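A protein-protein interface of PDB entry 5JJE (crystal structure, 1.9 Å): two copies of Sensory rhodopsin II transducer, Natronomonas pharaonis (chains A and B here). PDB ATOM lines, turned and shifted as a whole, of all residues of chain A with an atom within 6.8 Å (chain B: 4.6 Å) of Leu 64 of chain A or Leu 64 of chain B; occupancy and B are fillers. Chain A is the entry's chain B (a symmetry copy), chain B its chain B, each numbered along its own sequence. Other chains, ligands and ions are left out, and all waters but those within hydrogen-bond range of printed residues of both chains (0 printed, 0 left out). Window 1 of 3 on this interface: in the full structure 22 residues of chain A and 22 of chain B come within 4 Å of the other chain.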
ATOM      1  N   THR A  30      -0.514  -0.574  24.823  1.00  0.00           N
ATOM      2  CA  THR A  30      -1.494   0.404  25.265  1.00  0.00           C
ATOM      3  C   THR A  30      -1.139   1.804  24.762  1.00  0.00           C
ATOM      4  O   THR A  30      -2.002   2.529  24.276  1.00  0.00           O
ATOM      5  CB  THR A  30      -1.639   0.392  26.793  1.00  0.00           C
ATOM      6  OG1 THR A  30      -2.083  -0.903  27.204  1.00  0.00           O
ATOM      7  CG2 THR A  30      -2.659   1.431  27.248  1.00  0.00           C
ATOM      8  N   PHE A  33      -1.715   1.756  21.064  1.00  0.00           N
ATOM      9  CA  PHE A  33      -3.141   1.913  20.792  1.00  0.00           C
ATOM     10  C   PHE A  33      -3.591   3.361  21.057  1.00  0.00           C
ATOM     11  O   PHE A  33      -4.396   3.919  20.309  1.00  0.00           O
ATOM     12  CB  PHE A  33      -3.973   0.931  21.631  1.00  0.00           C
ATOM     13  CG  PHE A  33      -5.423   0.889  21.239  1.00  0.00           C
ATOM     14  CD1 PHE A  33      -5.872  -0.029  20.305  1.00  0.00           C
ATOM     15  CD2 PHE A  33      -6.332   1.785  21.783  1.00  0.00           C
ATOM     16  CE1 PHE A  33      -7.204  -0.058  19.926  1.00  0.00           C
ATOM     17  CE2 PHE A  33      -7.666   1.760  21.413  1.00  0.00           C
ATOM     18  CZ  PHE A  33      -8.102   0.834  20.477  1.00  0.00           C
ATOM     19  N   GLY A  34      -3.069   3.962  22.122  1.00  0.00           N
ATOM     20  CA  GLY A  34      -3.407   5.336  22.446  1.00  0.00           C
ATOM     21  C   GLY A  34      -2.935   6.297  21.372  1.00  0.00           C
ATOM     22  O   GLY A  34      -3.592   7.307  21.086  1.00  0.00           O
ATOM     23  N   ALA A  37      -5.367   5.965  18.395  1.00  0.00           N
ATOM     24  CA  ALA A  37      -6.558   6.707  18.792  1.00  0.00           C
ATOM     25  C   ALA A  37      -6.334   8.218  18.744  1.00  0.00           C
ATOM     26  O   ALA A  37      -7.171   8.965  18.229  1.00  0.00           O
ATOM     27  CB  ALA A  37      -6.983   6.282  20.200  1.00  0.00           C
ATOM     28  N   SER A  59     -15.093   6.499  19.749  1.00  0.00           N
ATOM     29  CA  SER A  59     -14.443   5.256  19.312  1.00  0.00           C
ATOM     30  C   SER A  59     -13.195   4.980  20.141  1.00  0.00           C
ATOM     31  O   SER A  59     -12.951   3.837  20.561  1.00  0.00           O
ATOM     32  CB  SER A  59     -14.083   5.364  17.827  1.00  0.00           C
ATOM     33  OG  SER A  59     -13.254   4.295  17.402  1.00  0.00           O
ATOM     34  N   ALA A  60     -12.398   6.020  20.368  1.00  0.00           N
ATOM     35  CA  ALA A  60     -11.176   5.892  21.159  1.00  0.00           C
ATOM     36  C   ALA A  60     -11.457   5.470  22.600  1.00  0.00           C
ATOM     37  O   ALA A  60     -10.729   4.657  23.175  1.00  0.00           O
ATOM     38  CB  ALA A  60     -10.390   7.179  21.139  1.00  0.00           C
ATOM     39  N   ILE A  61     -12.510   6.034  23.181  1.00  0.00           N
ATOM     40  CA  ILE A  61     -12.888   5.732  24.555  1.00  0.00           C
ATOM     41  C   ILE A  61     -13.398   4.303  24.694  1.00  0.00           C
ATOM     42  O   ILE A  61     -12.960   3.556  25.583  1.00  0.00           O
ATOM     43  CB  ILE A  61     -13.953   6.743  25.073  1.00  0.00           C
ATOM     44  CG1 ILE A  61     -13.294   8.099  25.318  1.00  0.00           C
ATOM     45  CG2 ILE A  61     -14.616   6.204  26.329  1.00  0.00           C
ATOM     46  CD1 ILE A  61     -14.290   9.292  25.475  1.00  0.00           C
ATOM     47  N   LEU A  62     -14.311   3.913  23.815  1.00  0.00           N
ATOM     48  CA  LEU A  62     -14.801   2.540  23.806  1.00  0.00           C
ATOM     49  C   LEU A  62     -13.646   1.564  23.555  1.00  0.00           C
ATOM     50  O   LEU A  62     -13.530   0.533  24.226  1.00  0.00           O
ATOM     51  CB  LEU A  62     -15.878   2.362  22.734  1.00  0.00           C
ATOM     52  CG  LEU A  62     -17.190   3.054  23.099  1.00  0.00           C
ATOM     53  CD1 LEU A  62     -18.200   2.944  21.964  1.00  0.00           C
ATOM     54  CD2 LEU A  62     -17.734   2.448  24.390  1.00  0.00           C
ATOM     55  N   GLY A  63     -12.786   1.915  22.609  1.00  0.00           N
ATOM     56  CA  GLY A  63     -11.661   1.072  22.245  1.00  0.00           C
ATOM     57  C   GLY A  63     -10.705   0.864  23.403  1.00  0.00           C
ATOM     58  O   GLY A  63     -10.228  -0.247  23.646  1.00  0.00           O
ATOM     59  N   LEU A  64     -10.414   1.942  24.124  1.00  0.00           N
ATOM     60  CA  LEU A  64      -9.523   1.861  25.275  1.00  0.00           C
ATOM     61  C   LEU A  64     -10.139   1.070  26.418  1.00  0.00           C
ATOM     62  O   LEU A  64      -9.429   0.362  27.140  1.00  0.00           O
ATOM     63  CB  LEU A  64      -9.095   3.258  25.732  1.00  0.00           C
ATOM     64  CG  LEU A  64      -8.042   3.875  24.811  1.00  0.00           C
ATOM     65  CD1 LEU A  64      -7.893   5.372  25.061  1.00  0.00           C
ATOM     66  CD2 LEU A  64      -6.707   3.170  24.998  1.00  0.00           C
ATOM     67  N   ILE A  65     -11.454   1.169  26.582  1.00  0.00           N
ATOM     68  CA  ILE A  65     -12.131   0.346  27.584  1.00  0.00           C
ATOM     69  C   ILE A  65     -12.031  -1.143  27.224  1.00  0.00           C
ATOM     70  O   ILE A  65     -11.741  -1.978  28.078  1.00  0.00           O
ATOM     71  CB  ILE A  65     -13.608   0.749  27.744  1.00  0.00           C
ATOM     72  CG1 ILE A  65     -13.699   2.121  28.414  1.00  0.00           C
ATOM     73  CG2 ILE A  65     -14.359  -0.272  28.580  1.00  0.00           C
ATOM     74  CD1 ILE A  65     -15.116   2.682  28.457  1.00  0.00           C
ATOM     75  N   ILE A  66     -12.256  -1.464  25.952  1.00  0.00           N
ATOM     76  CA  ILE A  66     -12.147  -2.851  25.501  1.00  0.00           C
ATOM     77  C   ILE A  66     -10.706  -3.346  25.681  1.00  0.00           C
ATOM     78  O   ILE A  66     -10.473  -4.469  26.131  1.00  0.00           O
ATOM     79  CB  ILE A  66     -12.613  -2.993  24.031  1.00  0.00           C
ATOM     80  CG1 ILE A  66     -14.127  -2.787  23.942  1.00  0.00           C
ATOM     81  CG2 ILE A  66     -12.270  -4.370  23.485  1.00  0.00           C
ATOM     82  CD1 ILE A  66     -14.614  -2.356  22.510  1.00  0.00           C
ATOM     83  N   LEU A  67      -9.748  -2.489  25.338  1.00  0.00           N
ATOM     84  CA  LEU A  67      -8.333  -2.790  25.514  1.00  0.00           C
ATOM     85  C   LEU A  67      -7.973  -3.155  26.965  1.00  0.00           C
ATOM     86  O   LEU A  67      -7.213  -4.105  27.196  1.00  0.00           O
ATOM     87  CB  LEU A  67      -7.469  -1.629  25.021  1.00  0.00           C
ATOM     88  CG  LEU A  67      -5.983  -1.949  24.857  1.00  0.00           C
ATOM     89  CD1 LEU A  67      -5.789  -2.822  23.644  1.00  0.00           C
ATOM     90  CD2 LEU A  67      -5.118  -0.698  24.757  1.00  0.00           C
ATOM     91  N   LEU A  68      -8.516  -2.423  27.938  1.00  0.00           N
ATOM     92  CA  LEU A  68      -8.340  -2.804  29.345  1.00  0.00           C
ATOM     93  C   LEU A  68      -8.812  -4.226  29.572  1.00  0.00           C
ATOM     94  O   LEU A  68      -8.124  -5.029  30.208  1.00  0.00           O
ATOM     95  CB  LEU A  68      -9.110  -1.887  30.309  1.00  0.00           C
ATOM     96  CG  LEU A  68      -9.317  -2.628  31.652  1.00  0.00           C
ATOM     97  CD1 LEU A  68      -8.086  -2.565  32.568  1.00  0.00           C
ATOM     98  CD2 LEU A  68     -10.574  -2.237  32.411  1.00  0.00           C
ATOM     99  N   GLY A  69      -9.994  -4.537  29.048  1.00  0.00           N
ATOM    100  CA  GLY A  69     -10.536  -5.878  29.169  1.00  0.00           C
ATOM    101  C   GLY A  69      -9.588  -6.922  28.609  1.00  0.00           C
ATOM    102  O   GLY A  69      -9.369  -7.973  29.215  1.00  0.00           O
ATOM    103  N   ASN A  71      -6.232  -6.601  28.120  1.00  0.00           N
ATOM    104  CA  ASN A  71      -5.011  -6.657  28.911  1.00  0.00           C
ATOM    105  C   ASN A  71      -5.254  -7.361  30.250  1.00  0.00           C
ATOM    106  O   ASN A  71      -4.458  -8.201  30.675  1.00  0.00           O
ATOM    107  CB  ASN A  71      -4.469  -5.258  29.171  1.00  0.00           C
ATOM    108  CG  ASN A  71      -4.048  -4.535  27.906  1.00  0.00           C
ATOM    109  OD1 ASN A  71      -3.719  -5.148  26.903  1.00  0.00           O
ATOM    110  ND2 ASN A  71      -4.034  -3.213  27.970  1.00  0.00           N
ATOM    111  N   PHE B  33     -15.427   5.619  34.683  1.00  0.00           N
ATOM    112  CA  PHE B  33     -14.445   6.581  34.190  1.00  0.00           C
ATOM    113  C   PHE B  33     -14.702   6.912  32.709  1.00  0.00           C
ATOM    114  O   PHE B  33     -14.577   8.063  32.288  1.00  0.00           O
ATOM    115  CB  PHE B  33     -13.014   6.057  34.382  1.00  0.00           C
ATOM    116  CG  PHE B  33     -11.957   7.085  34.099  1.00  0.00           C
ATOM    117  CD1 PHE B  33     -11.458   7.879  35.118  1.00  0.00           C
ATOM    118  CD2 PHE B  33     -11.481   7.278  32.810  1.00  0.00           C
ATOM    119  CE1 PHE B  33     -10.497   8.842  34.858  1.00  0.00           C
ATOM    120  CE2 PHE B  33     -10.518   8.237  32.542  1.00  0.00           C
ATOM    121  CZ  PHE B  33     -10.026   9.023  33.573  1.00  0.00           C
ATOM    122  N   ALA B  60      -9.137  12.412  27.820  1.00  0.00           N
ATOM    123  CA  ALA B  60      -9.795  11.119  28.001  1.00  0.00           C
ATOM    124  C   ALA B  60      -8.880   9.947  27.649  1.00  0.00           C
ATOM    125  O   ALA B  60      -8.877   8.920  28.333  1.00  0.00           O
ATOM    126  CB  ALA B  60     -11.064  11.048  27.189  1.00  0.00           C
ATOM    127  N   ILE B  61      -8.113  10.103  26.576  1.00  0.00           N
ATOM    128  CA  ILE B  61      -7.202   9.062  26.120  1.00  0.00           C
ATOM    129  C   ILE B  61      -6.045   8.864  27.093  1.00  0.00           C
ATOM    130  O   ILE B  61      -5.735   7.730  27.490  1.00  0.00           O
ATOM    131  CB  ILE B  61      -6.665   9.380  24.693  1.00  0.00           C
ATOM    132  CG1 ILE B  61      -7.776   9.164  23.669  1.00  0.00           C
ATOM    133  CG2 ILE B  61      -5.447   8.523  24.392  1.00  0.00           C
ATOM    134  CD1 ILE B  61      -7.505   9.794  22.266  1.00  0.00           C
ATOM    135  N   LEU B  62      -5.413   9.961  27.489  1.00  0.00           N
ATOM    136  CA  LEU B  62      -4.350   9.891  28.484  1.00  0.00           C
ATOM    137  C   LEU B  62      -4.887   9.313  29.798  1.00  0.00           C
ATOM    138  O   LEU B  62      -4.252   8.455  30.419  1.00  0.00           O
ATOM    139  CB  LEU B  62      -3.753  11.279  28.729  1.00  0.00           C
ATOM    140  CG  LEU B  62      -2.913  11.773  27.553  1.00  0.00           C
ATOM    141  CD1 LEU B  62      -2.424  13.196  27.790  1.00  0.00           C
ATOM    142  CD2 LEU B  62      -1.747  10.813  27.333  1.00  0.00           C
ATOM    143  N   GLY B  63      -6.068   9.770  30.192  1.00  0.00           N
ATOM    144  CA  GLY B  63      -6.684   9.331  31.432  1.00  0.00           C
ATOM    145  C   GLY B  63      -6.965   7.841  31.435  1.00  0.00           C
ATOM    146  O   GLY B  63      -6.725   7.148  32.426  1.00  0.00           O
ATOM    147  N   LEU B  64      -7.486   7.341  30.319  1.00  0.00           N
ATOM    148  CA  LEU B  64      -7.779   5.918  30.196  1.00  0.00           C
ATOM    149  C   LEU B  64      -6.514   5.075  30.170  1.00  0.00           C
ATOM    150  O   LEU B  64      -6.498   3.958  30.696  1.00  0.00           O
ATOM    151  CB  LEU B  64      -8.654   5.647  28.970  1.00  0.00           C
ATOM    152  CG  LEU B  64     -10.112   6.048  29.194  1.00  0.00           C
ATOM    153  CD1 LEU B  64     -10.881   6.111  27.878  1.00  0.00           C
ATOM    154  CD2 LEU B  64     -10.781   5.076  30.154  1.00  0.00           C
ATOM    155  N   ILE B  65      -5.448   5.604  29.577  1.00  0.00           N
ATOM    156  CA  ILE B  65      -4.165   4.902  29.618  1.00  0.00           C
ATOM    157  C   ILE B  65      -3.638   4.813  31.057  1.00  0.00           C
ATOM    158  O   ILE B  65      -3.178   3.760  31.494  1.00  0.00           O
ATOM    159  CB  ILE B  65      -3.119   5.583  28.717  1.00  0.00           C
ATOM    160  CG1 ILE B  65      -3.493   5.380  27.248  1.00  0.00           C
ATOM    161  CG2 ILE B  65      -1.735   5.011  28.970  1.00  0.00           C
ATOM    162  CD1 ILE B  65      -2.611   6.165  26.285  1.00  0.00           C
ATOM    163  N   ILE B  66      -3.725   5.918  31.792  1.00  0.00           N
ATOM    164  CA  ILE B  66      -3.286   5.925  33.187  1.00  0.00           C
ATOM    165  C   ILE B  66      -4.145   4.956  34.008  1.00  0.00           C
ATOM    166  O   ILE B  66      -3.633   4.203  34.841  1.00  0.00           O
ATOM    167  CB  ILE B  66      -3.332   7.358  33.775  1.00  0.00           C
ATOM    168  CG1 ILE B  66      -2.243   8.219  33.134  1.00  0.00           C
ATOM    169  CG2 ILE B  66      -3.118   7.331  35.281  1.00  0.00           C
ATOM    170  CD1 ILE B  66      -2.540   9.762  33.217  1.00  0.00           C
ATOM    171  N   LEU B  67      -5.450   4.973  33.753  1.00  0.00           N
ATOM    172  CA  LEU B  67      -6.384   4.063  34.405  1.00  0.00           C
ATOM    173  C   LEU B  67      -6.011   2.583  34.216  1.00  0.00           C
ATOM    174  O   LEU B  67      -6.081   1.798  35.172  1.00  0.00           O
ATOM    175  CB  LEU B  67      -7.813   4.323  33.927  1.00  0.00           C
ATOM    176  CG  LEU B  67      -8.908   3.661  34.763  1.00  0.00           C
ATOM    177  CD1 LEU B  67      -9.043   4.385  36.077  1.00  0.00           C
ATOM    178  CD2 LEU B  67     -10.251   3.611  34.042  1.00  0.00           C
ATOM    179  N   LEU B  68      -5.605   2.198  33.006  1.00  0.00           N
ATOM    180  CA  LEU B  68      -5.091   0.840  32.787  1.00  0.00           C
ATOM    181  C   LEU B  68      -3.940   0.552  33.729  1.00  0.00           C
ATOM    182  O   LEU B  68      -3.888  -0.504  34.364  1.00  0.00           O
ATOM    183  CB  LEU B  68      -4.597   0.617  31.349  1.00  0.00           C
ATOM    184  CG  LEU B  68      -3.619  -0.582  31.333  1.00  0.00           C
ATOM    185  CD1 LEU B  68      -4.335  -1.940  31.302  1.00  0.00           C
ATOM    186  CD2 LEU B  68      -2.543  -0.515  30.261  1.00  0.00           C
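The backbone carbonyl oxygen (O) of Leu 67 of chain A lies close to the side-chain amide nitrogen (ND2) of Asn 71 of chain A (3.4 Å).
The side-chain hydroxyl (OG1) of Thr 30 of chain A lies within hydrogen-bond range of the side-chain amide nitrogen (ND2) of Asn 71 of chain A (3.1 Å).
OG1 of Thr 30 of chain A touches CD2 of Leu 68 of chain B, at 3.1 Å.
Ile 61 of chain B touches Gly 34 of chain A.
Leu 64 of chain B touches Ile 61 of chain A.
Leu 64 of chain A touches Ile 61 of chain B.
CB of Leu 64 of chain A touches CD1 of Leu 64 of chain B (3.99 Å).
ND2 of Asn 71 of chain A touches CD1 of Leu 68 of chain B (3.6 Å).
Printed residues of chain B within 4 Å of Leu 64 of chain A: Ile 61 (3.9 Å) and Leu 64 (3.99 Å).
Printed residues of chain A within 4 Å of Leu 64 of chain B: Ile 61 and Leu 64.
Of the printed residues of chain B, Thr 30 of chain A touches Leu 68.
Of the printed residues of chain A, Ile 61 of chain B touches Gly 34 (3.98 Å) and Leu 64 (3.9 Å).
Of the printed residues of chain B, Gly 34 of chain A touches Ile 61 (3.98 Å).
Ala 60 of chain B touches none of the printed residues of chain A.
Leu 68 of chain A touches none of the printed residues of chain B.
Printed residues of chain B that touch a printed residue of chain A: Ile 61, Leu 64 and Leu 68.
Hydrophobic or aromatic side chains of chain B that line the printed part of chain A: Ile 61, Leu 64 and Leu 68.
Among the printed residues, 6 pairs touch across the chains.
Ile 61 of chain A touches Leu 64 of chain B, and with the chains exchanged Leu 64 of chain A touches Ile 61 of chain B.
Leu 64 of chain B touches its own counterpart, Leu 64 of chain A.
10 positions are printed for both chains.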
